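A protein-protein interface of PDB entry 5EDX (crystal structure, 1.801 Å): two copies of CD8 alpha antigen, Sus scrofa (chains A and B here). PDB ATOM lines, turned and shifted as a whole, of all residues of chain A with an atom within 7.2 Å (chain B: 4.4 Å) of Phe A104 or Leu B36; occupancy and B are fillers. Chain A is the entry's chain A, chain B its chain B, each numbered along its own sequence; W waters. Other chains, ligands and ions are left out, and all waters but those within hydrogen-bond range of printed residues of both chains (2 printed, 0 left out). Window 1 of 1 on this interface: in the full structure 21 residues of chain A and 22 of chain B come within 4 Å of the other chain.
Phe B104 touches Leu A36. Pro A46 touches Phe B93. Pro A46 touches Phe B104. Pro B46 touches Phe A93. CD2 of Phe B48 touches CG1 of Val A101, at 3.8 Å. Leu A102 touches Phe B48 (O to CB, 3.5 Å). CD1 of Leu A102 touches OG of Ser B95 (3.3 Å). Phe A104 touches Leu B36 (CZ to CD1, 3.9 Å). CD2 of Phe A104 touches O of Pro B46 (3.5 Å). Lys B45 touches Ser A105.
The side-chain amino group of Lys B45 is in hydrogen-bond range of the backbone carbonyl oxygen of Phe A104 (3.0 Å). The side-chain amide oxygen (OD1) of Asn A106 is in hydrogen-bond range of the side-chain amino group (NZ) of Lys B45.
Of the printed residues of chain B, Phe A104 touches Leu B36 (3.9 Å), Lys B45 (3.0 Å) and Pro B46 (3.5 Å). Of the printed residues of chain A, Leu B36 touches Phe A104. Of the printed residues of chain B, Phe A107 touches Lys B45. Of the printed residues of chain A, Pro B46 touches Phe A93 (3.8 Å) and Phe A104 (3.5 Å). Of the printed residues of chain B, Phe A93 touches Pro B46. Tyr B92 touches none of the printed residues of chain A. The nearest printed residue of chain B that does not touch Phe A104 is Phe B48 (4.5 Å). The nearest residue of chain A that does not touch Leu B36 is Leu A102 (4.5 Å). The nearest printed residue of chain B that does not touch Leu A102 is Leu B36 (4.5 Å).
The backbone NH of Leu A36 lies within hydrogen-bond range of the backbone carbonyl oxygen of Phe A93, at 2.7 Å. N of Ser A105 lies within hydrogen-bond range of O of Cys A94 (2.9 Å). O of Ser B34 is in hydrogen-bond range of N of Ser B95. The backbone carbonyl oxygen (O) of Phe B93 sits at hydrogen-bond distance from the backbone NH (N) of Leu B36 (2.7 Å).
Hydrophobic or aromatic side chains of chain B that line the printed part of chain A: Leu B36, Pro B46, Phe B48, Phe B93 and Phe B104.
Leu A36 touches Phe B104, and with the chains exchanged Phe A104 touches Leu B36. Pro A46 touches Phe B93, and with the chains exchanged Phe A93 touches Pro B46. Pro A46 touches Phe B104, and with the chains exchanged Phe A104 touches Pro B46.
Water W2 bridges OG of Ser B34 and N of Leu A102. Water W1 bridges N of Phe A107 (3.2 Å) and N of Lys B45 (3.3 Å).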
ATOM      1  N   LEU A   2      24.020  13.311  10.182  1.00  0.00           N
ATOM      2  CA  LEU A   2      25.334  13.076   9.597  1.00  0.00           C
ATOM      3  C   LEU A   2      25.674  14.117   8.528  1.00  0.00           C
ATOM      4  O   LEU A   2      26.823  14.561   8.420  1.00  0.00           O
ATOM      5  CB  LEU A   2      25.383  11.676   8.993  1.00  0.00           C
ATOM      6  CG  LEU A   2      26.670  11.308   8.252  1.00  0.00           C
ATOM      7  CD1 LEU A   2      27.856  11.286   9.204  1.00  0.00           C
ATOM      8  CD2 LEU A   2      26.519   9.977   7.553  1.00  0.00           C
ATOM      9  N   PHE A   3      24.669  14.491   7.738  1.00  0.00           N
ATOM     10  CA  PHE A   3      24.837  15.465   6.661  1.00  0.00           C
ATOM     11  C   PHE A   3      24.114  16.765   6.962  1.00  0.00           C
ATOM     12  O   PHE A   3      23.063  16.772   7.606  1.00  0.00           O
ATOM     13  CB  PHE A   3      24.227  14.943   5.359  1.00  0.00           C
ATOM     14  CG  PHE A   3      24.940  13.775   4.759  1.00  0.00           C
ATOM     15  CD1 PHE A   3      24.446  12.496   4.926  1.00  0.00           C
ATOM     16  CD2 PHE A   3      26.070  13.961   3.983  1.00  0.00           C
ATOM     17  CE1 PHE A   3      25.086  11.413   4.347  1.00  0.00           C
ATOM     18  CE2 PHE A   3      26.711  12.887   3.402  1.00  0.00           C
ATOM     19  CZ  PHE A   3      26.221  11.612   3.590  1.00  0.00           C
ATOM     20  N   LEU A  36      24.962  11.123  -5.826  1.00  0.00           N
ATOM     21  CA  LEU A  36      24.014  10.250  -6.507  1.00  0.00           C
ATOM     22  C   LEU A  36      22.862  11.084  -7.046  1.00  0.00           C
ATOM     23  O   LEU A  36      22.614  12.196  -6.591  1.00  0.00           O
ATOM     24  CB  LEU A  36      23.467   9.196  -5.545  1.00  0.00           C
ATOM     25  CG  LEU A  36      24.507   8.348  -4.810  1.00  0.00           C
ATOM     26  CD1 LEU A  36      23.813   7.398  -3.832  1.00  0.00           C
ATOM     27  CD2 LEU A  36      25.370   7.574  -5.804  1.00  0.00           C
ATOM     28  N   PRO A  46      19.020   4.701  -8.413  1.00  0.00           N
ATOM     29  CA  PRO A  46      19.917   5.857  -8.382  1.00  0.00           C
ATOM     30  C   PRO A  46      21.055   5.694  -9.377  1.00  0.00           C
ATOM     31  O   PRO A  46      21.433   4.576  -9.749  1.00  0.00           O
ATOM     32  CB  PRO A  46      20.484   5.825  -6.957  1.00  0.00           C
ATOM     33  CG  PRO A  46      19.536   5.010  -6.171  1.00  0.00           C
ATOM     34  CD  PRO A  46      18.975   3.998  -7.120  1.00  0.00           C
ATOM     35  N   PHE A  93      21.718  13.743  -4.169  1.00  0.00           N
ATOM     36  CA  PHE A  93      21.985  13.431  -2.770  1.00  0.00           C
ATOM     37  C   PHE A  93      23.342  12.776  -2.597  1.00  0.00           C
ATOM     38  O   PHE A  93      23.927  12.283  -3.559  1.00  0.00           O
ATOM     39  CB  PHE A  93      20.852  12.583  -2.154  1.00  0.00           C
ATOM     40  CG  PHE A  93      20.593  11.268  -2.853  1.00  0.00           C
ATOM     41  CD1 PHE A  93      20.026  11.231  -4.124  1.00  0.00           C
ATOM     42  CD2 PHE A  93      20.865  10.065  -2.212  1.00  0.00           C
ATOM     43  CE1 PHE A  93      19.767  10.014  -4.750  1.00  0.00           C
ATOM     44  CE2 PHE A  93      20.606   8.843  -2.831  1.00  0.00           C
ATOM     45  CZ  PHE A  93      20.054   8.820  -4.104  1.00  0.00           C
ATOM     46  N   CYS A  94      23.845  12.805  -1.367  1.00  0.00           N
ATOM     47  CA  CYS A  94      25.184  12.322  -1.071  1.00  0.00           C
ATOM     48  C   CYS A  94      25.104  11.005  -0.331  1.00  0.00           C
ATOM     49  O   CYS A  94      24.131  10.741   0.369  1.00  0.00           O
ATOM     50  CB  CYS A  94      25.930  13.342  -0.213  1.00  0.00           C
ATOM     51  SG  CYS A  94      26.203  14.906  -1.064  1.00  0.00           S
ATOM     52  N   SER A  95      26.117  10.192  -0.481  1.00  0.00           N
ATOM     53  CA  SER A  95      26.192   8.914   0.192  1.00  0.00           C
ATOM     54  C   SER A  95      27.575   8.683   0.821  1.00  0.00           C
ATOM     55  O   SER A  95      28.551   8.942   0.213  1.00  0.00           O
ATOM     56  CB  SER A  95      25.927   7.829  -0.812  1.00  0.00           C
ATOM     57  OG  SER A  95      25.629   6.661  -0.208  1.00  0.00           O
ATOM     58  N   PHE A  96      27.588   8.231   2.064  1.00  0.00           N
ATOM     59  CA  PHE A  96      28.791   8.157   2.918  1.00  0.00           C
ATOM     60  C   PHE A  96      28.771   6.778   3.577  1.00  0.00           C
ATOM     61  O   PHE A  96      27.736   6.295   3.972  1.00  0.00           O
ATOM     62  CB  PHE A  96      28.847   9.321   3.941  1.00  0.00           C
ATOM     63  CG  PHE A  96      29.893   9.185   4.977  1.00  0.00           C
ATOM     64  CD1 PHE A  96      31.221   9.496   4.688  1.00  0.00           C
ATOM     65  CD2 PHE A  96      29.584   8.747   6.232  1.00  0.00           C
ATOM     66  CE1 PHE A  96      32.195   9.362   5.645  1.00  0.00           C
ATOM     67  CE2 PHE A  96      30.549   8.596   7.184  1.00  0.00           C
ATOM     68  CZ  PHE A  96      31.866   8.899   6.897  1.00  0.00           C
ATOM     69  N   VAL A 101      27.779   0.479   6.979  1.00  0.00           N
ATOM     70  CA  VAL A 101      26.477   1.119   6.802  1.00  0.00           C
ATOM     71  C   VAL A 101      26.560   2.191   5.718  1.00  0.00           C
ATOM     72  O   VAL A 101      27.489   2.993   5.709  1.00  0.00           O
ATOM     73  CB  VAL A 101      25.970   1.771   8.104  1.00  0.00           C
ATOM     74  CG1 VAL A 101      24.668   2.537   7.852  1.00  0.00           C
ATOM     75  CG2 VAL A 101      25.779   0.720   9.197  1.00  0.00           C
ATOM     76  N   LEU A 102      25.596   2.190   4.801  1.00  0.00           N
ATOM     77  CA  LEU A 102      25.476   3.266   3.822  1.00  0.00           C
ATOM     78  C   LEU A 102      24.566   4.359   4.367  1.00  0.00           C
ATOM     79  O   LEU A 102      23.429   4.084   4.765  1.00  0.00           O
ATOM     80  CB  LEU A 102      24.899   2.740   2.504  1.00  0.00           C
ATOM     81  CG  LEU A 102      25.859   2.286   1.408  1.00  0.00           C
ATOM     82  CD1 LEU A 102      25.079   1.914   0.158  1.00  0.00           C
ATOM     83  CD2 LEU A 102      26.876   3.379   1.101  1.00  0.00           C
ATOM     84  N   TYR A 103      25.069   5.591   4.388  1.00  0.00           N
ATOM     85  CA  TYR A 103      24.302   6.740   4.841  1.00  0.00           C
ATOM     86  C   TYR A 103      23.942   7.633   3.664  1.00  0.00           C
ATOM     87  O   TYR A 103      24.728   7.780   2.734  1.00  0.00           O
ATOM     88  CB  TYR A 103      25.121   7.567   5.833  1.00  0.00           C
ATOM     89  CG  TYR A 103      25.406   6.855   7.134  1.00  0.00           C
ATOM     90  CD1 TYR A 103      24.575   7.022   8.228  1.00  0.00           C
ATOM     91  CD2 TYR A 103      26.503   6.014   7.261  1.00  0.00           C
ATOM     92  CE1 TYR A 103      24.829   6.370   9.424  1.00  0.00           C
ATOM     93  CE2 TYR A 103      26.765   5.357   8.451  1.00  0.00           C
ATOM     94  CZ  TYR A 103      25.925   5.541   9.525  1.00  0.00           C
ATOM     95  OH  TYR A 103      26.183   4.892  10.710  1.00  0.00           O
ATOM     96  N   PHE A 104      22.765   8.246   3.716  1.00  0.00           N
ATOM     97  CA  PHE A 104      22.330   9.123   2.628  1.00  0.00           C
ATOM     98  C   PHE A 104      21.907  10.482   3.153  1.00  0.00           C
ATOM     99  O   PHE A 104      21.235  10.564   4.174  1.00  0.00           O
ATOM    100  CB  PHE A 104      21.149   8.498   1.879  1.00  0.00           C
ATOM    101  CG  PHE A 104      21.432   7.127   1.347  1.00  0.00           C
ATOM    102  CD1 PHE A 104      22.089   6.960   0.141  1.00  0.00           C
ATOM    103  CD2 PHE A 104      21.041   6.001   2.051  1.00  0.00           C
ATOM    104  CE1 PHE A 104      22.352   5.696  -0.357  1.00  0.00           C
ATOM    105  CE2 PHE A 104      21.301   4.729   1.557  1.00  0.00           C
ATOM    106  CZ  PHE A 104      21.958   4.578   0.357  1.00  0.00           C
ATOM    107  N   SER A 105      22.279  11.549   2.447  1.00  0.00           N
ATOM    108  CA  SER A 105      21.760  12.874   2.769  1.00  0.00           C
ATOM    109  C   SER A 105      20.319  12.966   2.297  1.00  0.00           C
ATOM    110  O   SER A 105      19.889  12.181   1.456  1.00  0.00           O
ATOM    111  CB  SER A 105      22.570  13.970   2.073  1.00  0.00           C
ATOM    112  OG  SER A 105      22.219  14.062   0.700  1.00  0.00           O
ATOM    113  N   ASN A 106      19.581  13.931   2.834  1.00  0.00           N
ATOM    114  CA  ASN A 106      18.277  14.278   2.281  1.00  0.00           C
ATOM    115  C   ASN A 106      18.412  14.635   0.809  1.00  0.00           C
ATOM    116  O   ASN A 106      19.474  15.084   0.365  1.00  0.00           O
ATOM    117  CB  ASN A 106      17.679  15.475   3.023  1.00  0.00           C
ATOM    118  CG  ASN A 106      17.281  15.139   4.445  1.00  0.00           C
ATOM    119  OD1 ASN A 106      17.302  13.976   4.849  1.00  0.00           O
ATOM    120  ND2 ASN A 106      16.910  16.157   5.211  1.00  0.00           N
ATOM    121  N   PHE A 107      17.332  14.433   0.064  1.00  0.00           N
ATOM    122  CA  PHE A 107      17.260  14.839  -1.334  1.00  0.00           C
ATOM    123  C   PHE A 107      17.344  16.355  -1.473  1.00  0.00           C
ATOM    124  O   PHE A 107      16.734  17.097  -0.701  1.00  0.00           O
ATOM    125  CB  PHE A 107      15.930  14.380  -1.941  1.00  0.00           C
ATOM    126  CG  PHE A 107      15.931  12.959  -2.436  1.00  0.00           C
ATOM    127  CD1 PHE A 107      17.016  12.127  -2.222  1.00  0.00           C
ATOM    128  CD2 PHE A 107      14.833  12.459  -3.130  1.00  0.00           C
ATOM    129  CE1 PHE A 107      17.008  10.824  -2.686  1.00  0.00           C
ATOM    130  CE2 PHE A 107      14.821  11.159  -3.596  1.00  0.00           C
ATOM    131  CZ  PHE A 107      15.905  10.342  -3.381  1.00  0.00           C
ATOM    132  N   SER B  34      24.405  -4.392  -0.118  1.00  0.00           N
ATOM    133  CA  SER B  34      23.529  -3.763   0.862  1.00  0.00           C
ATOM    134  C   SER B  34      22.112  -3.744   0.318  1.00  0.00           C
ATOM    135  O   SER B  34      21.897  -3.381  -0.840  1.00  0.00           O
ATOM    136  CB  SER B  34      23.976  -2.332   1.167  1.00  0.00           C
ATOM    137  OG  SER B  34      25.271  -2.303   1.746  1.00  0.00           O
ATOM    138  N   TRP B  35      21.150  -4.145   1.141  1.00  0.00           N
ATOM    139  CA  TRP B  35      19.740  -4.028   0.766  1.00  0.00           C
ATOM    140  C   TRP B  35      19.225  -2.652   1.141  1.00  0.00           C
ATOM    141  O   TRP B  35      19.371  -2.215   2.285  1.00  0.00           O
ATOM    142  CB  TRP B  35      18.898  -5.105   1.458  1.00  0.00           C
ATOM    143  CG  TRP B  35      18.950  -6.433   0.770  1.00  0.00           C
ATOM    144  CD1 TRP B  35      19.652  -7.539   1.164  1.00  0.00           C
ATOM    145  CD2 TRP B  35      18.280  -6.789  -0.442  1.00  0.00           C
ATOM    146  NE1 TRP B  35      19.449  -8.567   0.269  1.00  0.00           N
ATOM    147  CE2 TRP B  35      18.614  -8.130  -0.727  1.00  0.00           C
ATOM    148  CE3 TRP B  35      17.423  -6.105  -1.313  1.00  0.00           C
ATOM    149  CZ2 TRP B  35      18.122  -8.800  -1.847  1.00  0.00           C
ATOM    150  CZ3 TRP B  35      16.936  -6.774  -2.426  1.00  0.00           C
ATOM    151  CH2 TRP B  35      17.286  -8.106  -2.683  1.00  0.00           C
ATOM    152  N   LEU B  36      18.612  -1.979   0.173  1.00  0.00           N
ATOM    153  CA  LEU B  36      18.068  -0.644   0.366  1.00  0.00           C
ATOM    154  C   LEU B  36      16.582  -0.620   0.021  1.00  0.00           C
ATOM    155  O   LEU B  36      16.090  -1.479  -0.706  1.00  0.00           O
ATOM    156  CB  LEU B  36      18.813   0.352  -0.519  1.00  0.00           C
ATOM    157  CG  LEU B  36      20.338   0.326  -0.424  1.00  0.00           C
ATOM    158  CD1 LEU B  36      20.947   1.249  -1.472  1.00  0.00           C
ATOM    159  CD2 LEU B  36      20.763   0.747   0.973  1.00  0.00           C
ATOM    160  N   TYR B  37      15.882   0.377   0.545  1.00  0.00           N
ATOM    161  CA  TYR B  37      14.441   0.500   0.364  1.00  0.00           C
ATOM    162  C   TYR B  37      14.079   1.950   0.076  1.00  0.00           C
ATOM    163  O   TYR B  37      14.663   2.868   0.654  1.00  0.00           O
ATOM    164  CB  TYR B  37      13.743   0.026   1.642  1.00  0.00           C
ATOM    165  CG  TYR B  37      12.273   0.366   1.760  1.00  0.00           C
ATOM    166  CD1 TYR B  37      11.300  -0.417   1.144  1.00  0.00           C
ATOM    167  CD2 TYR B  37      11.855   1.449   2.523  1.00  0.00           C
ATOM    168  CE1 TYR B  37       9.949  -0.112   1.270  1.00  0.00           C
ATOM    169  CE2 TYR B  37      10.515   1.761   2.656  1.00  0.00           C
ATOM    170  CZ  TYR B  37       9.568   0.985   2.029  1.00  0.00           C
ATOM    171  OH  TYR B  37       8.237   1.312   2.176  1.00  0.00           O
ATOM    172  N   LYS B  45      14.835  10.133   0.382  1.00  0.00           N
ATOM    173  CA  LYS B  45      16.061   9.351   0.344  1.00  0.00           C
ATOM    174  C   LYS B  45      15.847   7.878   0.669  1.00  0.00           C
ATOM    175  O   LYS B  45      14.966   7.531   1.460  1.00  0.00           O
ATOM    176  CB  LYS B  45      17.118   9.953   1.272  1.00  0.00           C
ATOM    177  CG  LYS B  45      16.792   9.922   2.749  1.00  0.00           C
ATOM    178  CD  LYS B  45      17.969  10.561   3.491  1.00  0.00           C
ATOM    179  CE  LYS B  45      17.703  10.782   4.959  1.00  0.00           C
ATOM    180  NZ  LYS B  45      18.793  11.633   5.531  1.00  0.00           N
ATOM    181  N   PRO B  46      16.668   7.008   0.061  1.00  0.00           N
ATOM    182  CA  PRO B  46      16.600   5.566   0.306  1.00  0.00           C
ATOM    183  C   PRO B  46      16.946   5.248   1.751  1.00  0.00           C
ATOM    184  O   PRO B  46      17.588   6.050   2.437  1.00  0.00           O
ATOM    185  CB  PRO B  46      17.693   4.992  -0.604  1.00  0.00           C
ATOM    186  CG  PRO B  46      18.109   6.091  -1.494  1.00  0.00           C
ATOM    187  CD  PRO B  46      17.801   7.366  -0.807  1.00  0.00           C
ATOM    188  N   ILE B  47      16.518   4.075   2.197  1.00  0.00           N
ATOM    189  CA  ILE B  47      16.723   3.635   3.569  1.00  0.00           C
ATOM    190  C   ILE B  47      17.587   2.388   3.565  1.00  0.00           C
ATOM    191  O   ILE B  47      17.320   1.434   2.836  1.00  0.00           O
ATOM    192  CB  ILE B  47      15.372   3.326   4.241  1.00  0.00           C
ATOM    193  CG1 ILE B  47      14.513   4.596   4.293  1.00  0.00           C
ATOM    194  CG2 ILE B  47      15.575   2.746   5.639  1.00  0.00           C
ATOM    195  CD1 ILE B  47      13.072   4.343   4.636  1.00  0.00           C
ATOM    196  N   PHE B  48      18.641   2.402   4.375  1.00  0.00           N
ATOM    197  CA  PHE B  48      19.528   1.260   4.495  1.00  0.00           C
ATOM    198  C   PHE B  48      18.860   0.194   5.361  1.00  0.00           C
ATOM    199  O   PHE B  48      18.379   0.493   6.463  1.00  0.00           O
ATOM    200  CB  PHE B  48      20.854   1.721   5.111  1.00  0.00           C
ATOM    201  CG  PHE B  48      21.781   0.603   5.498  1.00  0.00           C
ATOM    202  CD1 PHE B  48      22.581  -0.017   4.552  1.00  0.00           C
ATOM    203  CD2 PHE B  48      21.876   0.195   6.823  1.00  0.00           C
ATOM    204  CE1 PHE B  48      23.441  -1.042   4.915  1.00  0.00           C
ATOM    205  CE2 PHE B  48      22.739  -0.821   7.190  1.00  0.00           C
ATOM    206  CZ  PHE B  48      23.520  -1.441   6.238  1.00  0.00           C
ATOM    207  N   TYR B  91       9.760  -0.059  -2.738  1.00  0.00           N
ATOM    208  CA  TYR B  91      10.789  -0.446  -3.687  1.00  0.00           C
ATOM    209  C   TYR B  91      12.039  -0.939  -2.981  1.00  0.00           C
ATOM    210  O   TYR B  91      12.571  -0.260  -2.110  1.00  0.00           O
ATOM    211  CB  TYR B  91      11.131   0.747  -4.578  1.00  0.00           C
ATOM    212  CG  TYR B  91       9.910   1.291  -5.276  1.00  0.00           C
ATOM    213  CD1 TYR B  91       9.324   0.595  -6.329  1.00  0.00           C
ATOM    214  CD2 TYR B  91       9.322   2.478  -4.866  1.00  0.00           C
ATOM    215  CE1 TYR B  91       8.197   1.083  -6.968  1.00  0.00           C
ATOM    216  CE2 TYR B  91       8.191   2.974  -5.503  1.00  0.00           C
ATOM    217  CZ  TYR B  91       7.636   2.268  -6.547  1.00  0.00           C
ATOM    218  OH  TYR B  91       6.514   2.755  -7.183  1.00  0.00           O
ATOM    219  N   TYR B  92      12.497  -2.124  -3.367  1.00  0.00           N
ATOM    220  CA  TYR B  92      13.677  -2.740  -2.770  1.00  0.00           C
ATOM    221  C   TYR B  92      14.754  -2.929  -3.821  1.00  0.00           C
ATOM    222  O   TYR B  92      14.456  -3.272  -4.957  1.00  0.00           O
ATOM    223  CB  TYR B  92      13.310  -4.094  -2.162  1.00  0.00           C
ATOM    224  CG  TYR B  92      12.349  -3.987  -1.004  1.00  0.00           C
ATOM    225  CD1 TYR B  92      10.975  -3.901  -1.215  1.00  0.00           C
ATOM    226  CD2 TYR B  92      12.814  -3.962   0.298  1.00  0.00           C
ATOM    227  CE1 TYR B  92      10.095  -3.792  -0.147  1.00  0.00           C
ATOM    228  CE2 TYR B  92      11.948  -3.857   1.367  1.00  0.00           C
ATOM    229  CZ  TYR B  92      10.589  -3.777   1.139  1.00  0.00           C
ATOM    230  OH  TYR B  92       9.735  -3.671   2.215  1.00  0.00           O
ATOM    231  N   PHE B  93      16.010  -2.720  -3.435  1.00  0.00           N
ATOM    232  CA  PHE B  93      17.117  -2.855  -4.371  1.00  0.00           C
ATOM    233  C   PHE B  93      18.436  -3.070  -3.635  1.00  0.00           C
ATOM    234  O   PHE B  93      18.520  -2.883  -2.422  1.00  0.00           O
ATOM    235  CB  PHE B  93      17.201  -1.652  -5.327  1.00  0.00           C
ATOM    236  CG  PHE B  93      17.401  -0.318  -4.650  1.00  0.00           C
ATOM    237  CD1 PHE B  93      16.392   0.250  -3.884  1.00  0.00           C
ATOM    238  CD2 PHE B  93      18.579   0.397  -4.835  1.00  0.00           C
ATOM    239  CE1 PHE B  93      16.563   1.492  -3.293  1.00  0.00           C
ATOM    240  CE2 PHE B  93      18.760   1.639  -4.246  1.00  0.00           C
ATOM    241  CZ  PHE B  93      17.751   2.189  -3.473  1.00  0.00           C
ATOM    242  N   SER B  95      22.630  -2.269  -3.370  1.00  0.00           N
ATOM    243  CA  SER B  95      23.889  -1.735  -3.995  1.00  0.00           C
ATOM    244  C   SER B  95      25.281  -2.441  -3.686  1.00  0.00           C
ATOM    245  O   SER B  95      25.307  -3.178  -2.740  1.00  0.00           O
ATOM    246  CB  SER B  95      24.215  -0.301  -3.599  1.00  0.00           C
ATOM    247  OG  SER B  95      24.285  -0.179  -2.208  1.00  0.00           O
ATOM    248  N   PHE B 104      24.059  -0.183  -8.477  1.00  0.00           N
ATOM    249  CA  PHE B 104      22.718  -0.468  -7.965  1.00  0.00           C
ATOM    250  C   PHE B 104      21.977  -1.451  -8.862  1.00  0.00           C
ATOM    251  O   PHE B 104      22.098  -1.385 -10.087  1.00  0.00           O
ATOM    252  CB  PHE B 104      21.907   0.826  -7.854  1.00  0.00           C
ATOM    253  CG  PHE B 104      22.562   1.878  -7.001  1.00  0.00           C
ATOM    254  CD1 PHE B 104      22.391   1.878  -5.625  1.00  0.00           C
ATOM    255  CD2 PHE B 104      23.364   2.851  -7.571  1.00  0.00           C
ATOM    256  CE1 PHE B 104      22.999   2.845  -4.830  1.00  0.00           C
ATOM    257  CE2 PHE B 104      23.972   3.817  -6.785  1.00  0.00           C
ATOM    258  CZ  PHE B 104      23.793   3.811  -5.414  1.00  0.00           C
HETATM  259  O   HOH W   1      14.787  13.194   1.499  1.00  0.00           O
HETATM  260  O   HOH W   2      26.811  -0.541   3.313  1.00  0.00           O
